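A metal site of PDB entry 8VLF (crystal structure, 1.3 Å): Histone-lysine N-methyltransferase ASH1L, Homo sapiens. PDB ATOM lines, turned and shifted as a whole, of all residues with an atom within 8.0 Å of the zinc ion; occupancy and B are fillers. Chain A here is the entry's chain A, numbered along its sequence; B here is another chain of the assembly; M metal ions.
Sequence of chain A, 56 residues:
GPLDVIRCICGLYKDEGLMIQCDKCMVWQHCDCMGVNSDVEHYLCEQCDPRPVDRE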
ATOM      1  N   ARG A   7      11.486   8.420  -9.706  1.00  0.00           N
ATOM      2  CA  ARG A   7      11.264   8.436  -8.254  1.00  0.00           C
ATOM      3  C   ARG A   7      10.269   9.559  -7.970  1.00  0.00           C
ATOM      4  O   ARG A   7      10.662  10.684  -7.684  1.00  0.00           O
ATOM      5  CB  ARG A   7      12.536   8.627  -7.445  1.00  0.00           C
ATOM      6  CG  ARG A   7      12.270   8.347  -5.967  1.00  0.00           C
ATOM      7  CD  ARG A   7      13.280   8.977  -5.037  1.00  0.00           C
ATOM      8  NE  ARG A   7      13.309  10.435  -5.141  1.00  0.00           N
ATOM      9  CZ  ARG A   7      12.370  11.257  -4.674  1.00  0.00           C
ATOM     10  NH1 ARG A   7      11.283  10.780  -4.069  1.00  0.00           N
ATOM     11  NH2 ARG A   7      12.511  12.574  -4.817  1.00  0.00           N
ATOM     12  N   GLN A  21      12.154  16.227 -14.828  1.00  0.00           N
ATOM     13  CA  GLN A  21      13.390  15.768 -14.209  1.00  0.00           C
ATOM     14  C   GLN A  21      13.870  16.763 -13.166  1.00  0.00           C
ATOM     15  O   GLN A  21      13.881  17.975 -13.390  1.00  0.00           O
ATOM     16  CB  GLN A  21      14.472  15.585 -15.272  1.00  0.00           C
ATOM     17  CG  GLN A  21      15.785  15.083 -14.695  1.00  0.00           C
ATOM     18  CD  GLN A  21      16.765  14.671 -15.761  1.00  0.00           C
ATOM     19  OE1 GLN A  21      16.997  15.395 -16.730  1.00  0.00           O
ATOM     20  NE2 GLN A  21      17.330  13.477 -15.620  1.00  0.00           N
ATOM     21  N   CYS A  22      14.290  16.250 -12.014  1.00  0.00           N
ATOM     22  CA  CYS A  22      14.927  17.092 -11.013  1.00  0.00           C
ATOM     23  C   CYS A  22      16.259  17.605 -11.539  1.00  0.00           C
ATOM     24  O   CYS A  22      17.093  16.826 -12.029  1.00  0.00           O
ATOM     25  CB  CYS A  22      15.142  16.321  -9.706  1.00  0.00           C
ATOM     26  SG  CYS A  22      15.899  17.358  -8.390  1.00  0.00           S
ATOM     27  N   ASP A  23      16.459  18.922 -11.444  1.00  0.00           N
ATOM     28  CA  ASP A  23      17.679  19.540 -11.971  1.00  0.00           C
ATOM     29  C   ASP A  23      18.926  19.012 -11.287  1.00  0.00           C
ATOM     30  O   ASP A  23      20.010  19.021 -11.886  1.00  0.00           O
ATOM     31  CB  ASP A  23      17.617  21.053 -11.782  1.00  0.00           C
ATOM     32  CG  ASP A  23      16.680  21.722 -12.761  1.00  0.00           C
ATOM     33  OD1 ASP A  23      16.511  21.184 -13.875  1.00  0.00           O
ATOM     34  OD2 ASP A  23      16.149  22.792 -12.413  1.00  0.00           O
ATOM     35  N   LYS A  24      18.827  18.590 -10.021  1.00  0.00           N
ATOM     36  CA  LYS A  24      19.990  18.254  -9.218  1.00  0.00           C
ATOM     37  C   LYS A  24      20.248  16.754  -9.128  1.00  0.00           C
ATOM     38  O   LYS A  24      21.343  16.293  -9.489  1.00  0.00           O
ATOM     39  CB  LYS A  24      19.863  18.866  -7.815  1.00  0.00           C
ATOM     40  CG  LYS A  24      20.182  20.348  -7.768  1.00  0.00           C
ATOM     41  CD  LYS A  24      21.669  20.645  -7.890  1.00  0.00           C
ATOM     42  CE  LYS A  24      21.956  22.049  -7.394  1.00  0.00           C
ATOM     43  NZ  LYS A  24      23.325  22.488  -7.770  1.00  0.00           N
ATOM     44  N   CYS A  25      19.279  15.973  -8.649  1.00  0.00           N
ATOM     45  CA  CYS A  25      19.460  14.532  -8.467  1.00  0.00           C
ATOM     46  C   CYS A  25      19.067  13.702  -9.689  1.00  0.00           C
ATOM     47  O   CYS A  25      19.351  12.496  -9.718  1.00  0.00           O
ATOM     48  CB  CYS A  25      18.724  14.042  -7.210  1.00  0.00           C
ATOM     49  SG  CYS A  25      16.940  13.905  -7.392  1.00  0.00           S
ATOM     50  N   MET A  26      18.405  14.304 -10.674  1.00  0.00           N
ATOM     51  CA  MET A  26      18.104  13.706 -11.983  1.00  0.00           C
ATOM     52  C   MET A  26      16.980  12.679 -11.998  1.00  0.00           C
ATOM     53  O   MET A  26      16.747  12.078 -13.055  1.00  0.00           O
ATOM     54  CB  MET A  26      19.343  13.196 -12.745  1.00  0.00           C
ATOM     55  CG  MET A  26      20.526  14.134 -12.589  1.00  0.00           C
ATOM     56  SD  MET A  26      20.239  15.631 -13.550  1.00  0.00           S
ATOM     57  CE  MET A  26      20.194  14.998 -15.219  1.00  0.00           C
ATOM     58  N   VAL A  27      16.277  12.465 -10.888  1.00  0.00           N
ATOM     59  CA  VAL A  27      15.110  11.589 -10.948  1.00  0.00           C
ATOM     60  C   VAL A  27      13.992  12.228 -11.756  1.00  0.00           C
ATOM     61  O   VAL A  27      13.908  13.445 -11.920  1.00  0.00           O
ATOM     62  CB  VAL A  27      14.613  11.173  -9.554  1.00  0.00           C
ATOM     63  CG1 VAL A  27      15.738  10.569  -8.758  1.00  0.00           C
ATOM     64  CG2 VAL A  27      13.940  12.335  -8.818  1.00  0.00           C
ATOM     65  N   TRP A  28      13.123  11.378 -12.275  1.00  0.00           N
ATOM     66  CA  TRP A  28      11.949  11.798 -13.016  1.00  0.00           C
ATOM     67  C   TRP A  28      10.694  11.616 -12.152  1.00  0.00           C
ATOM     68  O   TRP A  28      10.560  10.608 -11.437  1.00  0.00           O
ATOM     69  CB  TRP A  28      11.807  10.966 -14.292  1.00  0.00           C
ATOM     70  CG  TRP A  28      12.871  11.250 -15.294  1.00  0.00           C
ATOM     71  CD1 TRP A  28      14.101  10.650 -15.384  1.00  0.00           C
ATOM     72  CD2 TRP A  28      12.826  12.226 -16.342  1.00  0.00           C
ATOM     73  NE1 TRP A  28      14.808  11.178 -16.430  1.00  0.00           N
ATOM     74  CE2 TRP A  28      14.053  12.151 -17.039  1.00  0.00           C
ATOM     75  CE3 TRP A  28      11.862  13.154 -16.779  1.00  0.00           C
ATOM     76  CZ2 TRP A  28      14.337  12.971 -18.127  1.00  0.00           C
ATOM     77  CZ3 TRP A  28      12.151  13.957 -17.853  1.00  0.00           C
ATOM     78  CH2 TRP A  28      13.377  13.854 -18.525  1.00  0.00           C
ATOM     79  N   GLN A  29       9.800  12.586 -12.232  1.00  0.00           N
ATOM     80  CA  GLN A  29       8.567  12.574 -11.465  1.00  0.00           C
ATOM     81  C   GLN A  29       7.404  12.895 -12.395  1.00  0.00           C
ATOM     82  O   GLN A  29       7.581  13.516 -13.449  1.00  0.00           O
ATOM     83  CB  GLN A  29       8.646  13.598 -10.330  1.00  0.00           C
ATOM     84  CG  GLN A  29       9.915  13.475  -9.509  1.00  0.00           C
ATOM     85  CD  GLN A  29       9.817  14.138  -8.145  1.00  0.00           C
ATOM     86  OE1 GLN A  29       9.647  15.350  -8.062  1.00  0.00           O
ATOM     87  NE2 GLN A  29       9.896  13.352  -7.072  1.00  0.00           N
ATOM     88  N   TYR A  43      13.266  22.958 -11.982  1.00  0.00           N
ATOM     89  CA  TYR A  43      12.506  22.025 -11.170  1.00  0.00           C
ATOM     90  C   TYR A  43      13.436  21.285 -10.218  1.00  0.00           C
ATOM     91  O   TYR A  43      14.491  20.782 -10.643  1.00  0.00           O
ATOM     92  CB  TYR A  43      11.749  21.004 -12.015  1.00  0.00           C
ATOM     93  CG  TYR A  43      10.919  20.113 -11.138  1.00  0.00           C
ATOM     94  CD1 TYR A  43       9.760  20.594 -10.535  1.00  0.00           C
ATOM     95  CD2 TYR A  43      11.326  18.823 -10.853  1.00  0.00           C
ATOM     96  CE1 TYR A  43       9.019  19.795  -9.698  1.00  0.00           C
ATOM     97  CE2 TYR A  43      10.585  18.025 -10.017  1.00  0.00           C
ATOM     98  CZ  TYR A  43       9.441  18.516  -9.441  1.00  0.00           C
ATOM     99  OH  TYR A  43       8.716  17.728  -8.600  1.00  0.00           O
ATOM    100  N   LEU A  44      13.021  21.176  -8.956  1.00  0.00           N
ATOM    101  CA  LEU A  44      13.637  20.294  -7.968  1.00  0.00           C
ATOM    102  C   LEU A  44      12.594  19.372  -7.363  1.00  0.00           C
ATOM    103  O   LEU A  44      11.453  19.773  -7.121  1.00  0.00           O
ATOM    104  CB  LEU A  44      14.274  21.115  -6.846  1.00  0.00           C
ATOM    105  CG  LEU A  44      15.492  21.953  -7.226  1.00  0.00           C
ATOM    106  CD1 LEU A  44      15.942  22.832  -6.052  1.00  0.00           C
ATOM    107  CD2 LEU A  44      16.634  21.097  -7.730  1.00  0.00           C
ATOM    108  N   CYS A  45      12.979  18.132  -7.103  1.00  0.00           N
ATOM    109  CA  CYS A  45      12.086  17.184  -6.458  1.00  0.00           C
ATOM    110  C   CYS A  45      11.851  17.570  -4.998  1.00  0.00           C
ATOM    111  O   CYS A  45      12.457  18.499  -4.459  1.00  0.00           O
ATOM    112  CB  CYS A  45      12.656  15.767  -6.593  1.00  0.00           C
ATOM    113  SG  CYS A  45      14.072  15.421  -5.531  1.00  0.00           S
ATOM    114  N   GLU A  46      10.958  16.812  -4.342  1.00  0.00           N
ATOM    115  CA  GLU A  46      10.550  17.047  -2.963  1.00  0.00           C
ATOM    116  C   GLU A  46      11.586  16.570  -1.946  1.00  0.00           C
ATOM    117  O   GLU A  46      11.443  16.886  -0.755  1.00  0.00           O
ATOM    118  CB  GLU A  46       9.188  16.379  -2.700  1.00  0.00           C
ATOM    119  CG  GLU A  46       9.225  14.934  -2.131  1.00  0.00           C
ATOM    120  CD  GLU A  46       9.758  13.898  -3.096  1.00  0.00           C
ATOM    121  OE1 GLU A  46      10.095  14.233  -4.251  1.00  0.00           O
ATOM    122  OE2 GLU A  46       9.824  12.716  -2.673  1.00  0.00           O
ATOM    123  N   GLN A  47      12.611  15.842  -2.369  1.00  0.00           N
ATOM    124  CA  GLN A  47      13.711  15.531  -1.453  1.00  0.00           C
ATOM    125  C   GLN A  47      14.802  16.588  -1.549  1.00  0.00           C
ATOM    126  O   GLN A  47      15.348  17.015  -0.526  1.00  0.00           O
ATOM    127  CB  GLN A  47      14.250  14.121  -1.739  1.00  0.00           C
ATOM    128  CG  GLN A  47      13.265  13.006  -1.402  1.00  0.00           C
ATOM    129  CD  GLN A  47      12.875  12.951   0.068  1.00  0.00           C
ATOM    130  OE1 GLN A  47      13.661  13.260   0.948  1.00  0.00           O
ATOM    131  NE2 GLN A  47      11.629  12.544   0.337  1.00  0.00           N
ATOM    132  N   CYS A  48      15.086  17.077  -2.763  1.00  0.00           N
ATOM    133  CA  CYS A  48      16.038  18.173  -2.917  1.00  0.00           C
ATOM    134  C   CYS A  48      15.490  19.476  -2.353  1.00  0.00           C
ATOM    135  O   CYS A  48      16.268  20.328  -1.901  1.00  0.00           O
ATOM    136  CB  CYS A  48      16.442  18.327  -4.393  1.00  0.00           C
ATOM    137  SG  CYS A  48      17.459  16.955  -5.029  1.00  0.00           S
ATOM    138  N   ASP A  49      14.166  19.668  -2.363  1.00  0.00           N
ATOM    139  CA  ASP A  49      13.524  20.894  -1.891  1.00  0.00           C
ATOM    140  C   ASP A  49      12.250  20.526  -1.143  1.00  0.00           C
ATOM    141  O   ASP A  49      11.139  20.578  -1.702  1.00  0.00           O
ATOM    142  CB  ASP A  49      13.227  21.827  -3.063  1.00  0.00           C
ATOM    143  CG  ASP A  49      12.703  23.175  -2.624  1.00  0.00           C
ATOM    144  OD1 ASP A  49      12.801  23.505  -1.417  1.00  0.00           O
ATOM    145  OD2 ASP A  49      12.184  23.899  -3.492  1.00  0.00           O
ATOM    146  N   ARG A  51       8.842  20.197   0.701  1.00  0.00           N
ATOM    147  CA  ARG A  51       7.683  21.078   0.669  1.00  0.00           C
ATOM    148  C   ARG A  51       6.413  20.252   0.683  1.00  0.00           C
ATOM    149  O   ARG A  51       6.421  19.075   0.308  1.00  0.00           O
ATOM    150  CB  ARG A  51       7.717  21.906  -0.613  1.00  0.00           C
ATOM    151  CG  ARG A  51       7.720  21.064  -1.865  1.00  0.00           C
ATOM    152  CD  ARG A  51       8.109  21.883  -3.096  1.00  0.00           C
ATOM    153  NE  ARG A  51       7.890  21.131  -4.325  1.00  0.00           N
ATOM    154  CZ  ARG A  51       8.839  20.452  -4.954  1.00  0.00           C
ATOM    155  NH1 ARG A  51      10.066  20.397  -4.447  1.00  0.00           N
ATOM    156  NH2 ARG A  51       8.574  19.801  -6.082  1.00  0.00           N
ATOM    157  N   PRO B   2      22.338  14.814  -0.460  1.00  0.00           N
ATOM    158  CA  PRO B   2      21.395  15.331  -1.468  1.00  0.00           C
ATOM    159  C   PRO B   2      21.589  14.788  -2.873  1.00  0.00           C
ATOM    160  O   PRO B   2      20.604  14.622  -3.597  1.00  0.00           O
ATOM    161  CB  PRO B   2      21.652  16.852  -1.417  1.00  0.00           C
ATOM    162  CG  PRO B   2      22.092  17.104  -0.018  1.00  0.00           C
ATOM    163  CD  PRO B   2      22.824  15.865   0.450  1.00  0.00           C
ATOM    164  N   LEU B   3      22.831  14.528  -3.286  1.00  0.00           N
ATOM    165  CA  LEU B   3      23.110  14.028  -4.620  1.00  0.00           C
ATOM    166  C   LEU B   3      22.950  12.525  -4.744  1.00  0.00           C
ATOM    167  O   LEU B   3      22.969  12.002  -5.864  1.00  0.00           O
ATOM    168  CB  LEU B   3      24.521  14.425  -5.050  1.00  0.00           C
ATOM    169  CG  LEU B   3      24.837  15.916  -4.930  1.00  0.00           C
ATOM    170  CD1 LEU B   3      26.346  16.149  -4.842  1.00  0.00           C
ATOM    171  CD2 LEU B   3      24.222  16.665  -6.085  1.00  0.00           C
ATOM    172  N   ASP B   4      22.804  11.807  -3.635  1.00  0.00           N
ATOM    173  CA  ASP B   4      22.604  10.359  -3.662  1.00  0.00           C
ATOM    174  C   ASP B   4      21.111  10.107  -3.688  1.00  0.00           C
ATOM    175  O   ASP B   4      20.357  10.712  -2.912  1.00  0.00           O
ATOM    176  CB  ASP B   4      23.201   9.710  -2.417  1.00  0.00           C
ATOM    177  CG  ASP B   4      24.668  10.044  -2.238  1.00  0.00           C
ATOM    178  OD1 ASP B   4      25.412  10.041  -3.245  1.00  0.00           O
ATOM    179  OD2 ASP B   4      25.088  10.278  -1.092  1.00  0.00           O
ATOM    180  N   VAL B   5      20.664   9.214  -4.569  1.00  0.00           N
ATOM    181  CA  VAL B   5      19.247   8.918  -4.711  1.00  0.00           C
ATOM    182  C   VAL B   5      18.951   7.624  -3.963  1.00  0.00           C
ATOM    183  O   VAL B   5      19.580   6.586  -4.224  1.00  0.00           O
ATOM    184  CB  VAL B   5      18.828   8.791  -6.192  1.00  0.00           C
ATOM    185  CG1 VAL B   5      17.348   8.389  -6.271  1.00  0.00           C
ATOM    186  CG2 VAL B   5      19.066  10.116  -6.933  1.00  0.00           C
ATOM    187  N   TYR B  13      12.157   7.152   1.919  1.00  0.00           N
ATOM    188  CA  TYR B  13      13.355   7.922   1.583  1.00  0.00           C
ATOM    189  C   TYR B  13      14.124   8.151   2.873  1.00  0.00           C
ATOM    190  O   TYR B  13      14.092   9.225   3.487  1.00  0.00           O
ATOM    191  CB  TYR B  13      13.015   9.236   0.880  1.00  0.00           C
ATOM    192  CG  TYR B  13      14.162   9.704   0.030  1.00  0.00           C
ATOM    193  CD1 TYR B  13      15.277  10.311   0.594  1.00  0.00           C
ATOM    194  CD2 TYR B  13      14.178   9.452  -1.346  1.00  0.00           C
ATOM    195  CE1 TYR B  13      16.347  10.712  -0.193  1.00  0.00           C
ATOM    196  CE2 TYR B  13      15.232   9.842  -2.137  1.00  0.00           C
ATOM    197  CZ  TYR B  13      16.323  10.456  -1.551  1.00  0.00           C
ATOM    198  OH  TYR B  13      17.378  10.824  -2.339  1.00  0.00           O
HETATM  199 ZN    ZN M   1      16.095  15.876  -6.584  1.00  0.00          ZN
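NH2 of Arg 7 lies close to SG of Cys 45 (3.3 Å).
SG of Cys 45 sits close to N of Gln 47 (3.5 Å).
The backbone carbonyl oxygen (O) of Cys 45 lies within hydrogen-bond range of the guanidinium group (NH1) of Arg 51.
The backbone NH of Cys 22 sits at hydrogen-bond distance from the backbone carbonyl oxygen of Val 27 (2.8 Å).
The side-chain sulfur (SG) of Cys 22 lies close to the backbone NH (N) of Lys 24 (3.6 Å).
SG of Cys 25 binds the zinc ion, at 2.3 Å.
SG of Cys 45 is bound to the zinc ion.
The side-chain sulfur (SG) of Cys 48 is bound to the zinc ion.
SG of Cys 22 is bound to the zinc ion (2.3 Å).
The zinc ion has four donor atoms within binding distance.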
